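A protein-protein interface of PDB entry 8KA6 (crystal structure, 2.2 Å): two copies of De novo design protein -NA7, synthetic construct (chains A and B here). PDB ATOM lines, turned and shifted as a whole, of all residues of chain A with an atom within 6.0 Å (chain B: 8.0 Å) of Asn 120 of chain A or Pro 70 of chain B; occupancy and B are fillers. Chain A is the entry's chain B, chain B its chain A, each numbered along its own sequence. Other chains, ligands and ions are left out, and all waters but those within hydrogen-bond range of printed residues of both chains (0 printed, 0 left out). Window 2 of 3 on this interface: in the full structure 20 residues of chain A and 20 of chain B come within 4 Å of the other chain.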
ATOM      1  N   GLU A 115     -14.198  21.539 -31.740  1.00  0.00           N
ATOM      2  CA  GLU A 115     -14.510  21.656 -30.319  1.00  0.00           C
ATOM      3  C   GLU A 115     -13.420  21.027 -29.462  1.00  0.00           C
ATOM      4  O   GLU A 115     -13.066  21.563 -28.403  1.00  0.00           O
ATOM      5  CB  GLU A 115     -15.857  20.996 -30.023  1.00  0.00           C
ATOM      6  CG  GLU A 115     -16.970  21.373 -30.981  1.00  0.00           C
ATOM      7  CD  GLU A 115     -17.488  22.774 -30.750  1.00  0.00           C
ATOM      8  OE1 GLU A 115     -17.136  23.377 -29.716  1.00  0.00           O
ATOM      9  OE2 GLU A 115     -18.250  23.274 -31.603  1.00  0.00           O
ATOM     10  N   LEU A 116     -12.889  19.883 -29.897  1.00  0.00           N
ATOM     11  CA  LEU A 116     -11.843  19.213 -29.132  1.00  0.00           C
ATOM     12  C   LEU A 116     -10.561  20.036 -29.115  1.00  0.00           C
ATOM     13  O   LEU A 116      -9.912  20.166 -28.070  1.00  0.00           O
ATOM     14  CB  LEU A 116     -11.583  17.824 -29.711  1.00  0.00           C
ATOM     15  CG  LEU A 116     -10.561  16.952 -28.977  1.00  0.00           C
ATOM     16  CD1 LEU A 116     -11.064  16.584 -27.588  1.00  0.00           C
ATOM     17  CD2 LEU A 116     -10.237  15.705 -29.783  1.00  0.00           C
ATOM     18  N   ALA A 117     -10.183  20.603 -30.263  1.00  0.00           N
ATOM     19  CA  ALA A 117      -8.972  21.412 -30.333  1.00  0.00           C
ATOM     20  C   ALA A 117      -9.140  22.768 -29.661  1.00  0.00           C
ATOM     21  O   ALA A 117      -8.137  23.418 -29.349  1.00  0.00           O
ATOM     22  CB  ALA A 117      -8.550  21.601 -31.790  1.00  0.00           C
ATOM     23  N   ALA A 118     -10.375  23.210 -29.438  1.00  0.00           N
ATOM     24  CA  ALA A 118     -10.637  24.488 -28.793  1.00  0.00           C
ATOM     25  C   ALA A 118     -10.714  24.380 -27.276  1.00  0.00           C
ATOM     26  O   ALA A 118     -10.878  25.403 -26.606  1.00  0.00           O
ATOM     27  CB  ALA A 118     -11.935  25.096 -29.330  1.00  0.00           C
ATOM     28  N   GLY A 119     -10.590  23.179 -26.720  1.00  0.00           N
ATOM     29  CA  GLY A 119     -10.686  23.019 -25.286  1.00  0.00           C
ATOM     30  C   GLY A 119     -12.096  23.260 -24.799  1.00  0.00           C
ATOM     31  O   GLY A 119     -12.316  23.985 -23.824  1.00  0.00           O
ATOM     32  N   ASN A 120     -13.064  22.657 -25.490  1.00  0.00           N
ATOM     33  CA  ASN A 120     -14.464  22.861 -25.141  1.00  0.00           C
ATOM     34  C   ASN A 120     -14.782  22.294 -23.765  1.00  0.00           C
ATOM     35  O   ASN A 120     -15.719  22.759 -23.105  1.00  0.00           O
ATOM     36  CB  ASN A 120     -15.356  22.226 -26.208  1.00  0.00           C
ATOM     37  CG  ASN A 120     -16.805  22.631 -26.071  1.00  0.00           C
ATOM     38  OD1 ASN A 120     -17.597  21.944 -25.427  1.00  0.00           O
ATOM     39  ND2 ASN A 120     -17.163  23.757 -26.679  1.00  0.00           N
ATOM     40  N   GLU A 121     -14.031  21.278 -23.330  1.00  0.00           N
ATOM     41  CA  GLU A 121     -14.149  20.669 -22.005  1.00  0.00           C
ATOM     42  C   GLU A 121     -15.483  19.954 -21.812  1.00  0.00           C
ATOM     43  O   GLU A 121     -15.584  19.037 -20.990  1.00  0.00           O
ATOM     44  CB  GLU A 121     -13.946  21.718 -20.907  1.00  0.00           C
ATOM     45  N   ASP A 122     -16.507  20.363 -22.553  1.00  0.00           N
ATOM     46  CA  ASP A 122     -17.814  19.709 -22.514  1.00  0.00           C
ATOM     47  C   ASP A 122     -17.936  18.730 -23.681  1.00  0.00           C
ATOM     48  O   ASP A 122     -18.769  18.873 -24.577  1.00  0.00           O
ATOM     49  CB  ASP A 122     -18.926  20.755 -22.539  1.00  0.00           C
ATOM     50  CG  ASP A 122     -20.207  20.260 -21.901  1.00  0.00           C
ATOM     51  OD1 ASP A 122     -20.221  19.115 -21.404  1.00  0.00           O
ATOM     52  OD2 ASP A 122     -21.200  21.019 -21.894  1.00  0.00           O
ATOM     53  N   LEU A 123     -17.065  17.717 -23.654  1.00  0.00           N
ATOM     54  CA  LEU A 123     -16.949  16.798 -24.781  1.00  0.00           C
ATOM     55  C   LEU A 123     -18.191  15.932 -24.948  1.00  0.00           C
ATOM     56  O   LEU A 123     -18.524  15.547 -26.074  1.00  0.00           O
ATOM     57  CB  LEU A 123     -15.709  15.918 -24.613  1.00  0.00           C
ATOM     58  CG  LEU A 123     -14.376  16.658 -24.507  1.00  0.00           C
ATOM     59  CD1 LEU A 123     -13.227  15.676 -24.335  1.00  0.00           C
ATOM     60  CD2 LEU A 123     -14.156  17.540 -25.728  1.00  0.00           C
ATOM     61  N   ALA A 125     -21.338  16.813 -24.504  1.00  0.00           N
ATOM     62  CA  ALA A 125     -22.290  17.588 -25.293  1.00  0.00           C
ATOM     63  C   ALA A 125     -21.830  17.711 -26.741  1.00  0.00           C
ATOM     64  O   ALA A 125     -22.646  17.629 -27.667  1.00  0.00           O
ATOM     65  CB  ALA A 125     -22.488  18.971 -24.672  1.00  0.00           C
ATOM     66  N   ALA A 126     -20.528  17.905 -26.957  1.00  0.00           N
ATOM     67  CA  ALA A 126     -20.014  17.990 -28.319  1.00  0.00           C
ATOM     68  C   ALA A 126     -20.135  16.652 -29.037  1.00  0.00           C
ATOM     69  O   ALA A 126     -20.528  16.603 -30.209  1.00  0.00           O
ATOM     70  CB  ALA A 126     -18.563  18.469 -28.302  1.00  0.00           C
ATOM     71  N   LEU B  66      -6.786  32.524 -27.671  1.00  0.00           N
ATOM     72  CA  LEU B  66      -7.781  32.311 -28.752  1.00  0.00           C
ATOM     73  C   LEU B  66      -8.781  31.259 -28.278  1.00  0.00           C
ATOM     74  O   LEU B  66      -9.845  31.124 -28.912  1.00  0.00           O
ATOM     75  CB  LEU B  66      -7.064  31.854 -30.022  1.00  0.00           C
ATOM     76  CG  LEU B  66      -7.626  32.394 -31.334  1.00  0.00           C
ATOM     77  CD1 LEU B  66      -6.623  33.320 -32.005  1.00  0.00           C
ATOM     78  CD2 LEU B  66      -7.996  31.254 -32.266  1.00  0.00           C
ATOM     79  N   LYS B  67      -8.455  30.556 -27.194  1.00  0.00           N
ATOM     80  CA  LYS B  67      -9.400  29.559 -26.627  1.00  0.00           C
ATOM     81  C   LYS B  67     -10.206  30.235 -25.514  1.00  0.00           C
ATOM     82  O   LYS B  67     -10.423  29.593 -24.466  1.00  0.00           O
ATOM     83  CB  LYS B  67      -8.657  28.357 -26.040  1.00  0.00           C
ATOM     84  CG  LYS B  67      -7.461  27.845 -26.826  1.00  0.00           C
ATOM     85  CD  LYS B  67      -6.507  27.055 -25.963  1.00  0.00           C
ATOM     86  CE  LYS B  67      -6.594  25.562 -26.190  1.00  0.00           C
ATOM     87  NZ  LYS B  67      -5.389  24.864 -25.686  1.00  0.00           N
ATOM     88  N   ASP B  69     -13.568  32.387 -25.851  1.00  0.00           N
ATOM     89  CA  ASP B  69     -14.968  31.982 -26.133  1.00  0.00           C
ATOM     90  C   ASP B  69     -14.918  30.689 -26.943  1.00  0.00           C
ATOM     91  O   ASP B  69     -14.500  30.750 -28.112  1.00  0.00           O
ATOM     92  CB  ASP B  69     -15.704  33.085 -26.888  1.00  0.00           C
ATOM     93  N   PRO B  70     -15.327  29.528 -26.389  1.00  0.00           N
ATOM     94  CA  PRO B  70     -15.175  28.258 -27.098  1.00  0.00           C
ATOM     95  C   PRO B  70     -16.100  28.130 -28.313  1.00  0.00           C
ATOM     96  O   PRO B  70     -15.698  27.534 -29.291  1.00  0.00           O
ATOM     97  CB  PRO B  70     -15.507  27.201 -26.036  1.00  0.00           C
ATOM     98  CG  PRO B  70     -16.395  27.920 -25.042  1.00  0.00           C
ATOM     99  CD  PRO B  70     -15.979  29.376 -25.087  1.00  0.00           C
ATOM    100  N   ALA B  71     -17.306  28.685 -28.227  1.00  0.00           N
ATOM    101  CA  ALA B  71     -18.265  28.532 -29.338  1.00  0.00           C
ATOM    102  C   ALA B  71     -17.842  29.454 -30.478  1.00  0.00           C
ATOM    103  O   ALA B  71     -18.154  29.153 -31.643  1.00  0.00           O
ATOM    104  CB  ALA B  71     -19.654  28.856 -28.861  1.00  0.00           C
ATOM    105  N   ARG B  72     -17.171  30.551 -30.137  1.00  0.00           N
ATOM    106  CA  ARG B  72     -16.694  31.483 -31.181  1.00  0.00           C
ATOM    107  C   ARG B  72     -15.554  30.794 -31.925  1.00  0.00           C
ATOM    108  O   ARG B  72     -15.467  30.953 -33.158  1.00  0.00           O
ATOM    109  CB  ARG B  72     -16.213  32.784 -30.533  1.00  0.00           C
ATOM    110  N   THR B  73     -14.732  30.044 -31.192  1.00  0.00           N
ATOM    111  CA  THR B  73     -13.587  29.397 -31.824  1.00  0.00           C
ATOM    112  C   THR B  73     -14.026  28.345 -32.836  1.00  0.00           C
ATOM    113  O   THR B  73     -13.297  28.071 -33.797  1.00  0.00           O
ATOM    114  CB  THR B  73     -12.686  28.781 -30.748  1.00  0.00           C
ATOM    115  OG1 THR B  73     -12.236  29.809 -29.854  1.00  0.00           O
ATOM    116  CG2 THR B  73     -11.471  28.105 -31.369  1.00  0.00           C
ATOM    117  N   ALA B  74     -15.222  27.777 -32.659  1.00  0.00           N
ATOM    118  CA  ALA B  74     -15.690  26.698 -33.525  1.00  0.00           C
ATOM    119  C   ALA B  74     -15.679  27.111 -34.992  1.00  0.00           C
ATOM    120  O   ALA B  74     -15.007  26.488 -35.821  1.00  0.00           O
ATOM    121  CB  ALA B  74     -17.092  26.257 -33.098  1.00  0.00           C
ATOM    122  N   ALA B  75     -16.422  28.167 -35.331  1.00  0.00           N
ATOM    123  CA  ALA B  75     -16.446  28.641 -36.710  1.00  0.00           C
ATOM    124  C   ALA B  75     -15.109  29.224 -37.146  1.00  0.00           C
ATOM    125  O   ALA B  75     -14.868  29.356 -38.352  1.00  0.00           O
ATOM    126  CB  ALA B  75     -17.549  29.685 -36.891  1.00  0.00           C
ATOM    127  N   LEU B  76     -14.239  29.573 -36.199  1.00  0.00           N
ATOM    128  CA  LEU B  76     -12.939  30.127 -36.555  1.00  0.00           C
ATOM    129  C   LEU B  76     -11.970  29.032 -36.986  1.00  0.00           C
ATOM    130  O   LEU B  76     -11.169  29.236 -37.906  1.00  0.00           O
ATOM    131  CB  LEU B  76     -12.369  30.919 -35.379  1.00  0.00           C
ATOM    132  CG  LEU B  76     -11.179  31.832 -35.683  1.00  0.00           C
ATOM    133  CD1 LEU B  76     -11.493  32.746 -36.857  1.00  0.00           C
ATOM    134  CD2 LEU B  76     -10.821  32.646 -34.453  1.00  0.00           C
ATOM    135  N   VAL B  77     -12.027  27.870 -36.334  1.00  0.00           N
ATOM    136  CA  VAL B  77     -11.196  26.744 -36.748  1.00  0.00           C
ATOM    137  C   VAL B  77     -11.622  26.247 -38.124  1.00  0.00           C
ATOM    138  O   VAL B  77     -10.781  25.900 -38.962  1.00  0.00           O
ATOM    139  CB  VAL B  77     -11.253  25.622 -35.695  1.00  0.00           C
ATOM    140  CG1 VAL B  77     -10.466  24.406 -36.161  1.00  0.00           C
ATOM    141  CG2 VAL B  77     -10.716  26.117 -34.363  1.00  0.00           C
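No position is printed for both chains.
Of the 11 printed residues of chain A, 3 touch a printed residue of chain B. Hydrophobic or aromatic side chains of chain A within 4 Å of the printed part of chain B: Ala 118. Among the printed residues, no Asp or Glu carboxylate lies within 4 Å of a Lys or Arg side-chain nitrogen of the other chain.
Glu 115 of chain A touches Ala 74 of chain B (OE2 to CB, 3.5 Å). Ala 118 of chain A touches Lys 67 of chain B (O to CB, 3.7 Å). Ala 118 of chain A touches Thr 73 of chain B (CB to CG2, 3.7 Å). Asn 120 of chain A touches Pro 70 of chain B (ND2 to CB, 3.9 Å).
Of the printed residues of chain B, Glu 115 of chain A touches Ala 74 (3.5 Å). Ala 117 of chain A touches none of the printed residues of chain B. Printed residues of chain B within 4 Å of Ala 118 of chain A: Lys 67 (3.7 Å) and Thr 73 (3.7 Å). No residue of chain B comes within 4 Å of Gly 119 of chain A. Of chain B, only Pro 70 (3.9 Å) comes within 4 Å of Asn 120 of chain A. Of the printed residues of chain A, Lys 67 of chain B touches Ala 118. Pro 70 of chain B touches just one residue of chain A: Asn 120. Printed residues of chain A within 4 Å of Thr 73 of chain B: Ala 118 (3.7 Å). Of the printed residues of chain A, Ala 74 of chain B touches Glu 115 (3.5 Å). Leu 76 of chain B touches none of the printed residues of chain A.
OG1 of Thr 73 of chain B sits at hydrogen-bond distance from O of Leu 66 of chain B (2.9 Å). OG1 of Thr 73 of chain B is in hydrogen-bond range of O of Asp 69 of chain B. The side-chain carboxylate of Glu 115 of chain A lies within hydrogen-bond range of the side-chain amide nitrogen of Asn 120 of chain A (3.1 Å). The backbone carbonyl oxygen (O) of Asp 122 of chain A sits close to the side-chain amide oxygen (OD1) of Asn 120 of chain A (3.4 Å).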
